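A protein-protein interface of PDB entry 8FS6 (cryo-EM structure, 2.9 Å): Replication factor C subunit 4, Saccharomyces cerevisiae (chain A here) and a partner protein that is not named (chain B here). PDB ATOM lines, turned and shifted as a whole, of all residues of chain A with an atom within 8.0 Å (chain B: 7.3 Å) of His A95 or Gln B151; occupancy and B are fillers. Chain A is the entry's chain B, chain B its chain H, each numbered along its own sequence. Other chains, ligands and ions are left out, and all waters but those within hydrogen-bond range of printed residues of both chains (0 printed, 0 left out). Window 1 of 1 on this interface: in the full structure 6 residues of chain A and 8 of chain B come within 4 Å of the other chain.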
ATOM      1  N   LEU A  76     -21.783 -13.475 -16.061  1.00  0.00           N
ATOM      2  CA  LEU A  76     -22.346 -13.306 -17.399  1.00  0.00           C
ATOM      3  C   LEU A  76     -22.735 -11.838 -17.537  1.00  0.00           C
ATOM      4  O   LEU A  76     -23.805 -11.424 -17.079  1.00  0.00           O
ATOM      5  CB  LEU A  76     -23.542 -14.227 -17.624  1.00  0.00           C
ATOM      6  CG  LEU A  76     -24.281 -14.054 -18.952  1.00  0.00           C
ATOM      7  CD1 LEU A  76     -23.379 -14.429 -20.117  1.00  0.00           C
ATOM      8  CD2 LEU A  76     -25.560 -14.876 -18.973  1.00  0.00           C
ATOM      9  N   VAL A  88     -32.682 -14.104 -25.941  1.00  0.00           N
ATOM     10  CA  VAL A  88     -31.443 -14.230 -25.182  1.00  0.00           C
ATOM     11  C   VAL A  88     -31.740 -14.523 -23.717  1.00  0.00           C
ATOM     12  O   VAL A  88     -31.093 -15.379 -23.104  1.00  0.00           O
ATOM     13  CB  VAL A  88     -30.573 -12.973 -25.364  1.00  0.00           C
ATOM     14  CG1 VAL A  88     -29.812 -12.635 -24.088  1.00  0.00           C
ATOM     15  CG2 VAL A  88     -29.603 -13.185 -26.515  1.00  0.00           C
ATOM     16  N   VAL A  89     -32.744 -13.855 -23.144  1.00  0.00           N
ATOM     17  CA  VAL A  89     -33.138 -14.137 -21.766  1.00  0.00           C
ATOM     18  C   VAL A  89     -33.609 -15.581 -21.630  1.00  0.00           C
ATOM     19  O   VAL A  89     -33.277 -16.270 -20.657  1.00  0.00           O
ATOM     20  CB  VAL A  89     -34.218 -13.141 -21.304  1.00  0.00           C
ATOM     21  CG1 VAL A  89     -34.763 -13.537 -19.941  1.00  0.00           C
ATOM     22  CG2 VAL A  89     -33.651 -11.732 -21.255  1.00  0.00           C
ATOM     23  N   ARG A  90     -34.375 -16.067 -22.608  1.00  0.00           N
ATOM     24  CA  ARG A  90     -34.914 -17.417 -22.534  1.00  0.00           C
ATOM     25  C   ARG A  90     -33.879 -18.500 -22.811  1.00  0.00           C
ATOM     26  O   ARG A  90     -34.095 -19.651 -22.416  1.00  0.00           O
ATOM     27  CB  ARG A  90     -36.085 -17.570 -23.508  1.00  0.00           C
ATOM     28  CG  ARG A  90     -37.382 -16.955 -23.008  1.00  0.00           C
ATOM     29  CD  ARG A  90     -38.540 -17.249 -23.946  1.00  0.00           C
ATOM     30  NE  ARG A  90     -38.239 -16.874 -25.322  1.00  0.00           N
ATOM     31  CZ  ARG A  90     -39.154 -16.701 -26.267  1.00  0.00           C
ATOM     32  NH1 ARG A  90     -40.443 -16.851 -26.015  1.00  0.00           N
ATOM     33  NH2 ARG A  90     -38.764 -16.367 -27.493  1.00  0.00           N
ATOM     34  N   ASN A  91     -32.769 -18.178 -23.478  1.00  0.00           N
ATOM     35  CA  ASN A  91     -31.778 -19.195 -23.812  1.00  0.00           C
ATOM     36  C   ASN A  91     -30.460 -19.020 -23.066  1.00  0.00           C
ATOM     37  O   ASN A  91     -30.084 -19.888 -22.276  1.00  0.00           O
ATOM     38  CB  ASN A  91     -31.527 -19.192 -25.327  1.00  0.00           C
ATOM     39  CG  ASN A  91     -32.567 -19.984 -26.091  1.00  0.00           C
ATOM     40  OD1 ASN A  91     -33.226 -20.862 -25.536  1.00  0.00           O
ATOM     41  ND2 ASN A  91     -32.721 -19.677 -27.374  1.00  0.00           N
ATOM     42  N   GLN A  92     -29.765 -17.897 -23.255  1.00  0.00           N
ATOM     43  CA  GLN A  92     -28.417 -17.756 -22.713  1.00  0.00           C
ATOM     44  C   GLN A  92     -28.439 -17.560 -21.201  1.00  0.00           C
ATOM     45  O   GLN A  92     -27.680 -18.212 -20.473  1.00  0.00           O
ATOM     46  CB  GLN A  92     -27.700 -16.590 -23.396  1.00  0.00           C
ATOM     47  CG  GLN A  92     -26.247 -16.422 -22.982  1.00  0.00           C
ATOM     48  CD  GLN A  92     -25.589 -15.231 -23.649  1.00  0.00           C
ATOM     49  OE1 GLN A  92     -26.215 -14.522 -24.438  1.00  0.00           O
ATOM     50  NE2 GLN A  92     -24.319 -15.005 -23.337  1.00  0.00           N
ATOM     51  N   ILE A  93     -29.308 -16.671 -20.715  1.00  0.00           N
ATOM     52  CA  ILE A  93     -29.418 -16.449 -19.277  1.00  0.00           C
ATOM     53  C   ILE A  93     -29.938 -17.702 -18.588  1.00  0.00           C
ATOM     54  O   ILE A  93     -29.480 -18.066 -17.498  1.00  0.00           O
ATOM     55  CB  ILE A  93     -30.313 -15.228 -18.990  1.00  0.00           C
ATOM     56  CG1 ILE A  93     -29.805 -14.006 -19.756  1.00  0.00           C
ATOM     57  CG2 ILE A  93     -30.360 -14.938 -17.497  1.00  0.00           C
ATOM     58  CD1 ILE A  93     -30.527 -12.721 -19.411  1.00  0.00           C
ATOM     59  N   LYS A  94     -30.897 -18.388 -19.217  1.00  0.00           N
ATOM     60  CA  LYS A  94     -31.426 -19.622 -18.646  1.00  0.00           C
ATOM     61  C   LYS A  94     -30.350 -20.697 -18.552  1.00  0.00           C
ATOM     62  O   LYS A  94     -30.244 -21.389 -17.533  1.00  0.00           O
ATOM     63  CB  LYS A  94     -32.610 -20.117 -19.475  1.00  0.00           C
ATOM     64  CG  LYS A  94     -33.054 -21.531 -19.138  1.00  0.00           C
ATOM     65  CD  LYS A  94     -34.266 -21.943 -19.955  1.00  0.00           C
ATOM     66  CE  LYS A  94     -35.409 -22.385 -19.057  1.00  0.00           C
ATOM     67  NZ  LYS A  94     -35.916 -23.735 -19.423  1.00  0.00           N
ATOM     68  N   HIS A  95     -29.532 -20.848 -19.598  1.00  0.00           N
ATOM     69  CA  HIS A  95     -28.487 -21.866 -19.570  1.00  0.00           C
ATOM     70  C   HIS A  95     -27.372 -21.504 -18.599  1.00  0.00           C
ATOM     71  O   HIS A  95     -26.775 -22.399 -17.988  1.00  0.00           O
ATOM     72  CB  HIS A  95     -27.926 -22.081 -20.976  1.00  0.00           C
ATOM     73  CG  HIS A  95     -28.915 -22.669 -21.934  1.00  0.00           C
ATOM     74  ND1 HIS A  95     -30.100 -23.240 -21.522  1.00  0.00           N
ATOM     75  CD2 HIS A  95     -28.898 -22.771 -23.284  1.00  0.00           C
ATOM     76  CE1 HIS A  95     -30.769 -23.669 -22.576  1.00  0.00           C
ATOM     77  NE2 HIS A  95     -30.062 -23.397 -23.658  1.00  0.00           N
ATOM     78  N   PHE A  96     -27.069 -20.213 -18.444  1.00  0.00           N
ATOM     79  CA  PHE A  96     -26.087 -19.811 -17.443  1.00  0.00           C
ATOM     80  C   PHE A  96     -26.609 -20.037 -16.030  1.00  0.00           C
ATOM     81  O   PHE A  96     -25.838 -20.412 -15.139  1.00  0.00           O
ATOM     82  CB  PHE A  96     -25.699 -18.346 -17.639  1.00  0.00           C
ATOM     83  CG  PHE A  96     -24.701 -17.845 -16.633  1.00  0.00           C
ATOM     84  CD1 PHE A  96     -23.375 -18.238 -16.702  1.00  0.00           C
ATOM     85  CD2 PHE A  96     -25.088 -16.984 -15.621  1.00  0.00           C
ATOM     86  CE1 PHE A  96     -22.453 -17.782 -15.780  1.00  0.00           C
ATOM     87  CE2 PHE A  96     -24.171 -16.524 -14.696  1.00  0.00           C
ATOM     88  CZ  PHE A  96     -22.852 -16.923 -14.775  1.00  0.00           C
ATOM     89  N   ALA A  97     -27.905 -19.810 -15.804  1.00  0.00           N
ATOM     90  CA  ALA A  97     -28.490 -20.076 -14.496  1.00  0.00           C
ATOM     91  C   ALA A  97     -28.539 -21.572 -14.205  1.00  0.00           C
ATOM     92  O   ALA A  97     -28.321 -21.995 -13.063  1.00  0.00           O
ATOM     93  CB  ALA A  97     -29.889 -19.467 -14.416  1.00  0.00           C
ATOM     94  N   GLN A  98     -28.822 -22.385 -15.223  1.00  0.00           N
ATOM     95  CA  GLN A  98     -28.886 -23.832 -15.060  1.00  0.00           C
ATOM     96  C   GLN A  98     -27.515 -24.476 -14.915  1.00  0.00           C
ATOM     97  O   GLN A  98     -27.443 -25.667 -14.594  1.00  0.00           O
ATOM     98  CB  GLN A  98     -29.620 -24.466 -16.244  1.00  0.00           C
ATOM     99  CG  GLN A  98     -31.118 -24.222 -16.250  1.00  0.00           C
ATOM    100  CD  GLN A  98     -31.798 -24.809 -17.472  1.00  0.00           C
ATOM    101  OE1 GLN A  98     -31.225 -24.839 -18.561  1.00  0.00           O
ATOM    102  NE2 GLN A  98     -33.028 -25.279 -17.296  1.00  0.00           N
ATOM    103  N   LYS A  99     -26.437 -23.732 -15.152  1.00  0.00           N
ATOM    104  CA  LYS A  99     -25.100 -24.278 -14.983  1.00  0.00           C
ATOM    105  C   LYS A  99     -24.856 -24.631 -13.520  1.00  0.00           C
ATOM    106  O   LYS A  99     -25.316 -23.943 -12.605  1.00  0.00           O
ATOM    107  CB  LYS A  99     -24.051 -23.278 -15.475  1.00  0.00           C
ATOM    108  CG  LYS A  99     -22.677 -23.880 -15.720  1.00  0.00           C
ATOM    109  CD  LYS A  99     -21.818 -22.965 -16.579  1.00  0.00           C
ATOM    110  CE  LYS A  99     -21.666 -21.590 -15.947  1.00  0.00           C
ATOM    111  NZ  LYS A  99     -20.645 -20.767 -16.651  1.00  0.00           N
ATOM    112  N   LYS A 100     -24.120 -25.718 -13.305  1.00  0.00           N
ATOM    113  CA  LYS A 100     -23.894 -26.279 -11.976  1.00  0.00           C
ATOM    114  C   LYS A 100     -22.435 -26.155 -11.554  1.00  0.00           C
ATOM    115  O   LYS A 100     -21.837 -27.100 -11.038  1.00  0.00           O
ATOM    116  CB  LYS A 100     -24.340 -27.737 -11.917  1.00  0.00           C
ATOM    117  CG  LYS A 100     -24.989 -28.117 -10.597  1.00  0.00           C
ATOM    118  CD  LYS A 100     -26.150 -29.069 -10.800  1.00  0.00           C
ATOM    119  CE  LYS A 100     -27.242 -28.425 -11.632  1.00  0.00           C
ATOM    120  NZ  LYS A 100     -27.747 -27.157 -11.041  1.00  0.00           N
ATOM    121  N   LYS A 109     -23.155 -17.398  -8.528  1.00  0.00           N
ATOM    122  CA  LYS A 109     -22.953 -16.826  -9.850  1.00  0.00           C
ATOM    123  C   LYS A 109     -23.655 -15.476  -9.946  1.00  0.00           C
ATOM    124  O   LYS A 109     -24.715 -15.259  -9.355  1.00  0.00           O
ATOM    125  CB  LYS A 109     -23.474 -17.772 -10.931  1.00  0.00           C
ATOM    126  CG  LYS A 109     -22.734 -19.099 -11.003  1.00  0.00           C
ATOM    127  CD  LYS A 109     -23.363 -20.033 -12.025  1.00  0.00           C
ATOM    128  CE  LYS A 109     -24.845 -20.235 -11.752  1.00  0.00           C
ATOM    129  NZ  LYS A 109     -25.455 -21.207 -12.700  1.00  0.00           N
ATOM    130  N   THR A 130     -36.898 -16.096 -14.540  1.00  0.00           N
ATOM    131  CA  THR A 130     -35.510 -16.542 -14.491  1.00  0.00           C
ATOM    132  C   THR A 130     -34.939 -16.405 -13.078  1.00  0.00           C
ATOM    133  O   THR A 130     -34.315 -17.335 -12.555  1.00  0.00           O
ATOM    134  CB  THR A 130     -34.679 -15.756 -15.507  1.00  0.00           C
ATOM    135  OG1 THR A 130     -34.888 -16.307 -16.812  1.00  0.00           O
ATOM    136  CG2 THR A 130     -33.213 -15.895 -15.199  1.00  0.00           C
ATOM    137  N   TYR A 134     -34.413 -19.967 -10.713  1.00  0.00           N
ATOM    138  CA  TYR A 134     -32.990 -20.134 -10.431  1.00  0.00           C
ATOM    139  C   TYR A 134     -32.489 -18.962  -9.589  1.00  0.00           C
ATOM    140  O   TYR A 134     -31.887 -18.006 -10.076  1.00  0.00           O
ATOM    141  CB  TYR A 134     -32.210 -20.278 -11.731  1.00  0.00           C
ATOM    142  CG  TYR A 134     -32.794 -21.308 -12.671  1.00  0.00           C
ATOM    143  CD1 TYR A 134     -32.742 -22.661 -12.364  1.00  0.00           C
ATOM    144  CD2 TYR A 134     -33.404 -20.929 -13.859  1.00  0.00           C
ATOM    145  CE1 TYR A 134     -33.277 -23.608 -13.215  1.00  0.00           C
ATOM    146  CE2 TYR A 134     -33.943 -21.869 -14.717  1.00  0.00           C
ATOM    147  CZ  TYR A 134     -33.877 -23.207 -14.390  1.00  0.00           C
ATOM    148  OH  TYR A 134     -34.410 -24.149 -15.240  1.00  0.00           O
ATOM    149  N   ASP B  29     -35.788 -30.177 -21.868  1.00  0.00           N
ATOM    150  CA  ASP B  29     -34.601 -30.855 -21.370  1.00  0.00           C
ATOM    151  C   ASP B  29     -34.865 -32.350 -21.252  1.00  0.00           C
ATOM    152  O   ASP B  29     -35.926 -32.770 -20.780  1.00  0.00           O
ATOM    153  CB  ASP B  29     -34.176 -30.289 -20.013  1.00  0.00           C
ATOM    154  CG  ASP B  29     -33.513 -28.930 -20.131  1.00  0.00           C
ATOM    155  OD1 ASP B  29     -34.190 -27.973 -20.563  1.00  0.00           O
ATOM    156  OD2 ASP B  29     -32.316 -28.820 -19.794  1.00  0.00           O
ATOM    157  N   PHE B  94     -28.722 -37.590 -15.096  1.00  0.00           N
ATOM    158  CA  PHE B  94     -28.377 -36.215 -15.420  1.00  0.00           C
ATOM    159  C   PHE B  94     -29.397 -35.653 -16.398  1.00  0.00           C
ATOM    160  O   PHE B  94     -30.048 -36.397 -17.137  1.00  0.00           O
ATOM    161  CB  PHE B  94     -26.958 -36.107 -16.004  1.00  0.00           C
ATOM    162  CG  PHE B  94     -26.744 -36.919 -17.253  1.00  0.00           C
ATOM    163  CD1 PHE B  94     -26.375 -38.253 -17.174  1.00  0.00           C
ATOM    164  CD2 PHE B  94     -26.891 -36.344 -18.505  1.00  0.00           C
ATOM    165  CE1 PHE B  94     -26.171 -39.000 -18.319  1.00  0.00           C
ATOM    166  CE2 PHE B  94     -26.689 -37.086 -19.653  1.00  0.00           C
ATOM    167  CZ  PHE B  94     -26.327 -38.415 -19.559  1.00  0.00           C
ATOM    168  N   ARG B  95     -29.528 -34.330 -16.395  1.00  0.00           N
ATOM    169  CA  ARG B  95     -30.465 -33.622 -17.258  1.00  0.00           C
ATOM    170  C   ARG B  95     -29.687 -32.802 -18.278  1.00  0.00           C
ATOM    171  O   ARG B  95     -28.829 -31.996 -17.909  1.00  0.00           O
ATOM    172  CB  ARG B  95     -31.386 -32.715 -16.440  1.00  0.00           C
ATOM    173  CG  ARG B  95     -32.493 -32.068 -17.254  1.00  0.00           C
ATOM    174  CD  ARG B  95     -33.043 -30.820 -16.577  1.00  0.00           C
ATOM    175  NE  ARG B  95     -32.854 -30.833 -15.131  1.00  0.00           N
ATOM    176  CZ  ARG B  95     -32.348 -29.825 -14.435  1.00  0.00           C
ATOM    177  NH1 ARG B  95     -31.960 -28.705 -15.023  1.00  0.00           N
ATOM    178  NH2 ARG B  95     -32.231 -29.941 -13.115  1.00  0.00           N
ATOM    179  N   VAL B  96     -29.996 -33.006 -19.557  1.00  0.00           N
ATOM    180  CA  VAL B  96     -29.320 -32.320 -20.649  1.00  0.00           C
ATOM    181  C   VAL B  96     -30.375 -31.701 -21.557  1.00  0.00           C
ATOM    182  O   VAL B  96     -31.499 -32.203 -21.666  1.00  0.00           O
ATOM    183  CB  VAL B  96     -28.390 -33.280 -21.435  1.00  0.00           C
ATOM    184  CG1 VAL B  96     -29.195 -34.346 -22.169  1.00  0.00           C
ATOM    185  CG2 VAL B  96     -27.475 -32.517 -22.389  1.00  0.00           C
ATOM    186  N   ASN B  97     -30.017 -30.581 -22.186  1.00  0.00           N
ATOM    187  CA  ASN B  97     -30.938 -29.891 -23.079  1.00  0.00           C
ATOM    188  C   ASN B  97     -31.263 -30.761 -24.287  1.00  0.00           C
ATOM    189  O   ASN B  97     -30.367 -31.318 -24.928  1.00  0.00           O
ATOM    190  CB  ASN B  97     -30.336 -28.560 -23.529  1.00  0.00           C
ATOM    191  CG  ASN B  97     -31.348 -27.663 -24.215  1.00  0.00           C
ATOM    192  OD1 ASN B  97     -32.542 -27.962 -24.251  1.00  0.00           O
ATOM    193  ND2 ASN B  97     -30.873 -26.552 -24.767  1.00  0.00           N
ATOM    194  N   ARG B  99     -32.696 -29.828 -27.233  1.00  0.00           N
ATOM    195  CA  ARG B  99     -32.323 -29.208 -28.500  1.00  0.00           C
ATOM    196  C   ARG B  99     -30.820 -29.281 -28.731  1.00  0.00           C
ATOM    197  O   ARG B  99     -30.368 -29.475 -29.866  1.00  0.00           O
ATOM    198  CB  ARG B  99     -32.801 -27.757 -28.535  1.00  0.00           C
ATOM    199  CG  ARG B  99     -34.313 -27.601 -28.535  1.00  0.00           C
ATOM    200  CD  ARG B  99     -34.723 -26.136 -28.518  1.00  0.00           C
ATOM    201  NE  ARG B  99     -34.420 -25.491 -27.246  1.00  0.00           N
ATOM    202  CZ  ARG B  99     -33.392 -24.681 -27.041  1.00  0.00           C
ATOM    203  NH1 ARG B  99     -32.540 -24.386 -28.009  1.00  0.00           N
ATOM    204  NH2 ARG B  99     -33.212 -24.151 -25.834  1.00  0.00           N
ATOM    205  N   HIS B 100     -30.028 -29.123 -27.668  1.00  0.00           N
ATOM    206  CA  HIS B 100     -28.580 -29.223 -27.803  1.00  0.00           C
ATOM    207  C   HIS B 100     -28.151 -30.654 -28.107  1.00  0.00           C
ATOM    208  O   HIS B 100     -27.176 -30.875 -28.834  1.00  0.00           O
ATOM    209  CB  HIS B 100     -27.898 -28.714 -26.534  1.00  0.00           C
ATOM    210  CG  HIS B 100     -27.996 -27.232 -26.348  1.00  0.00           C
ATOM    211  ND1 HIS B 100     -28.783 -26.431 -27.148  1.00  0.00           N
ATOM    212  CD2 HIS B 100     -27.403 -26.404 -25.454  1.00  0.00           C
ATOM    213  CE1 HIS B 100     -28.672 -25.174 -26.754  1.00  0.00           C
ATOM    214  NE2 HIS B 100     -27.840 -25.132 -25.728  1.00  0.00           N
ATOM    215  N   ALA B 131     -15.751 -31.063 -16.036  1.00  0.00           N
ATOM    216  CA  ALA B 131     -16.624 -31.299 -14.895  1.00  0.00           C
ATOM    217  C   ALA B 131     -17.996 -30.695 -15.158  1.00  0.00           C
ATOM    218  O   ALA B 131     -18.102 -29.548 -15.610  1.00  0.00           O
ATOM    219  CB  ALA B 131     -16.015 -30.707 -13.625  1.00  0.00           C
ATOM    220  N   ASN B 132     -19.045 -31.473 -14.879  1.00  0.00           N
ATOM    221  CA  ASN B 132     -20.429 -31.107 -15.190  1.00  0.00           C
ATOM    222  C   ASN B 132     -20.615 -30.819 -16.678  1.00  0.00           C
ATOM    223  O   ASN B 132     -21.482 -30.032 -17.066  1.00  0.00           O
ATOM    224  CB  ASN B 132     -20.901 -29.915 -14.347  1.00  0.00           C
ATOM    225  CG  ASN B 132     -21.095 -30.275 -12.888  1.00  0.00           C
ATOM    226  OD1 ASN B 132     -21.398 -31.421 -12.554  1.00  0.00           O
ATOM    227  ND2 ASN B 132     -20.921 -29.295 -12.010  1.00  0.00           N
ATOM    228  N   ARG B 133     -19.802 -31.457 -17.518  1.00  0.00           N
ATOM    229  CA  ARG B 133     -19.875 -31.310 -18.968  1.00  0.00           C
ATOM    230  C   ARG B 133     -19.910 -32.701 -19.586  1.00  0.00           C
ATOM    231  O   ARG B 133     -18.951 -33.467 -19.452  1.00  0.00           O
ATOM    232  CB  ARG B 133     -18.690 -30.506 -19.507  1.00  0.00           C
ATOM    233  CG  ARG B 133     -18.497 -29.150 -18.849  1.00  0.00           C
ATOM    234  CD  ARG B 133     -19.283 -28.068 -19.571  1.00  0.00           C
ATOM    235  NE  ARG B 133     -18.847 -26.731 -19.184  1.00  0.00           N
ATOM    236  CZ  ARG B 133     -17.807 -26.100 -19.713  1.00  0.00           C
ATOM    237  NH1 ARG B 133     -17.069 -26.657 -20.660  1.00  0.00           N
ATOM    238  NH2 ARG B 133     -17.501 -24.880 -19.280  1.00  0.00           N
ATOM    239  N   LEU B 134     -21.012 -33.024 -20.256  1.00  0.00           N
ATOM    240  CA  LEU B 134     -21.131 -34.306 -20.933  1.00  0.00           C
ATOM    241  C   LEU B 134     -20.187 -34.354 -22.128  1.00  0.00           C
ATOM    242  O   LEU B 134     -20.030 -33.369 -22.852  1.00  0.00           O
ATOM    243  CB  LEU B 134     -22.575 -34.526 -21.383  1.00  0.00           C
ATOM    244  CG  LEU B 134     -22.994 -35.924 -21.834  1.00  0.00           C
ATOM    245  CD1 LEU B 134     -22.823 -36.928 -20.706  1.00  0.00           C
ATOM    246  CD2 LEU B 134     -24.436 -35.898 -22.314  1.00  0.00           C
ATOM    247  N   CYS B 149     -19.086 -30.726 -25.873  1.00  0.00           N
ATOM    248  CA  CYS B 149     -19.157 -30.729 -24.412  1.00  0.00           C
ATOM    249  C   CYS B 149     -20.410 -29.998 -23.945  1.00  0.00           C
ATOM    250  O   CYS B 149     -20.330 -28.889 -23.403  1.00  0.00           O
ATOM    251  CB  CYS B 149     -17.900 -30.103 -23.805  1.00  0.00           C
ATOM    252  SG  CYS B 149     -16.412 -31.117 -23.960  1.00  0.00           S
ATOM    253  N   PRO B 150     -21.590 -30.590 -24.138  1.00  0.00           N
ATOM    254  CA  PRO B 150     -22.802 -29.989 -23.573  1.00  0.00           C
ATOM    255  C   PRO B 150     -22.838 -30.155 -22.063  1.00  0.00           C
ATOM    256  O   PRO B 150     -22.442 -31.191 -21.523  1.00  0.00           O
ATOM    257  CB  PRO B 150     -23.936 -30.767 -24.250  1.00  0.00           C
ATOM    258  CG  PRO B 150     -23.333 -32.085 -24.567  1.00  0.00           C
ATOM    259  CD  PRO B 150     -21.898 -31.808 -24.911  1.00  0.00           C
ATOM    260  N   GLN B 151     -23.317 -29.120 -21.380  1.00  0.00           N
ATOM    261  CA  GLN B 151     -23.437 -29.178 -19.933  1.00  0.00           C
ATOM    262  C   GLN B 151     -24.618 -30.056 -19.532  1.00  0.00           C
ATOM    263  O   GLN B 151     -25.583 -30.224 -20.283  1.00  0.00           O
ATOM    264  CB  GLN B 151     -23.592 -27.770 -19.352  1.00  0.00           C
ATOM    265  CG  GLN B 151     -25.030 -27.333 -19.109  1.00  0.00           C
ATOM    266  CD  GLN B 151     -25.216 -25.837 -19.254  1.00  0.00           C
ATOM    267  OE1 GLN B 151     -24.257 -25.098 -19.483  1.00  0.00           O
ATOM    268  NE2 GLN B 151     -26.456 -25.380 -19.124  1.00  0.00           N
ATOM    269  N   PHE B 152     -24.526 -30.639 -18.338  1.00  0.00           N
ATOM    270  CA  PHE B 152     -25.597 -31.461 -17.797  1.00  0.00           C
ATOM    271  C   PHE B 152     -25.833 -31.106 -16.337  1.00  0.00           C
ATOM    272  O   PHE B 152     -24.951 -30.588 -15.647  1.00  0.00           O
ATOM    273  CB  PHE B 152     -25.300 -32.968 -17.945  1.00  0.00           C
ATOM    274  CG  PHE B 152     -24.122 -33.453 -17.138  1.00  0.00           C
ATOM    275  CD1 PHE B 152     -24.281 -33.880 -15.827  1.00  0.00           C
ATOM    276  CD2 PHE B 152     -22.861 -33.510 -17.702  1.00  0.00           C
ATOM    277  CE1 PHE B 152     -23.203 -34.334 -15.093  1.00  0.00           C
ATOM    278  CE2 PHE B 152     -21.779 -33.967 -16.973  1.00  0.00           C
ATOM    279  CZ  PHE B 152     -21.950 -34.377 -15.667  1.00  0.00           C
ATOM    280  N   GLN B 153     -27.046 -31.393 -15.876  1.00  0.00           N
ATOM    281  CA  GLN B 153     -27.451 -31.156 -14.497  1.00  0.00           C
ATOM    282  C   GLN B 153     -27.843 -32.479 -13.856  1.00  0.00           C
ATOM    283  O   GLN B 153     -28.836 -33.094 -14.283  1.00  0.00           O
ATOM    284  CB  GLN B 153     -28.614 -30.165 -14.436  1.00  0.00           C
ATOM    285  CG  GLN B 153     -28.295 -28.797 -15.021  1.00  0.00           C
ATOM    286  CD  GLN B 153     -28.720 -28.660 -16.467  1.00  0.00           C
ATOM    287  OE1 GLN B 153     -29.911 -28.590 -16.771  1.00  0.00           O
ATOM    288  NE2 GLN B 153     -27.748 -28.620 -17.370  1.00  0.00           N
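Of the printed residues of chain B, Asn A91 touches Arg B99 (3.3 Å).
Of chain B, only Asn B97, Arg B99, His B100 and Gln B151 come within 4 Å of His A95.
Ala A97 touches none of the printed residues of chain B.
Of the printed residues of chain B, Gln A98 touches Gln B153.
Tyr A134 touches none of the printed residues of chain B.
Printed residues of chain A within 4 Å of Asn B97: His A95.
Printed residues of chain A within 4 Å of His B100: His A95.
Of chain A, only His A95 comes within 4 Å of Gln B151.
Printed residues of chain A within 4 Å of Gln B153: Gln A98 and Lys A100.
The nearest residue of chain A that does not touch Gln B151 is Lys A99 (4.3 Å).
The nearest printed residue of chain B that does not touch Lys A100 is Phe B152 (4.7 Å).
Among the printed residues, pairs that only touch across the chains: His A95 with Arg B99 (3.9 Å), Gln A98 with Gln B153 (3.3 Å) and Lys A100 with Gln B153 (3.6 Å).
The side-chain amide oxygen (OD1) of Asn A91 lies within hydrogen-bond range of the guanidinium group (NH2) of Arg B99.
The side-chain amide nitrogen (ND2) of Asn B97 is in hydrogen-bond range of a ring nitrogen (NE2) of His A95 (3.4 Å).
NE2 of His B100 sits at hydrogen-bond distance from NE2 of His A95 (3.5 Å).
The backbone carbonyl oxygen (O) of His A95 sits at hydrogen-bond distance from the side-chain amide nitrogen (NE2) of Gln B151 (3.2 Å).
The backbone carbonyl oxygen (O) of Lys A100 lies within hydrogen-bond range of the side-chain amide nitrogen (ND2) of Asn B132.
O of Asn A91 lies close to ND1 of His A95, 3.4 Å away.
The side-chain hydroxyl (OH) of Tyr A134 lies within hydrogen-bond range of the side-chain amide nitrogen (NE2) of Gln A98 (2.7 Å).
N of Arg B95 lies within hydrogen-bond range of O of Gln B153, 2.5 Å away.
The side-chain amide nitrogen (ND2) of Asn B97 is in hydrogen-bond range of a ring nitrogen (ND1) of His B100.
The backbone carbonyl oxygen (O) of Asn B132 lies within hydrogen-bond range of the backbone NH (N) of Phe B152 (3.4 Å).
Of the 17 printed residues of chain A, 4 touch a printed residue of chain B.
Hydrophobic or aromatic side chains of chain B that line the printed part of chain A: His B100.
Along chain B the printed residues that touch a printed residue of chain A span positions 97 to 153.
Among the printed residues, no Asp or Glu carboxylate lies within 4 Å of a Lys or Arg side-chain nitrogen of the other chain.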
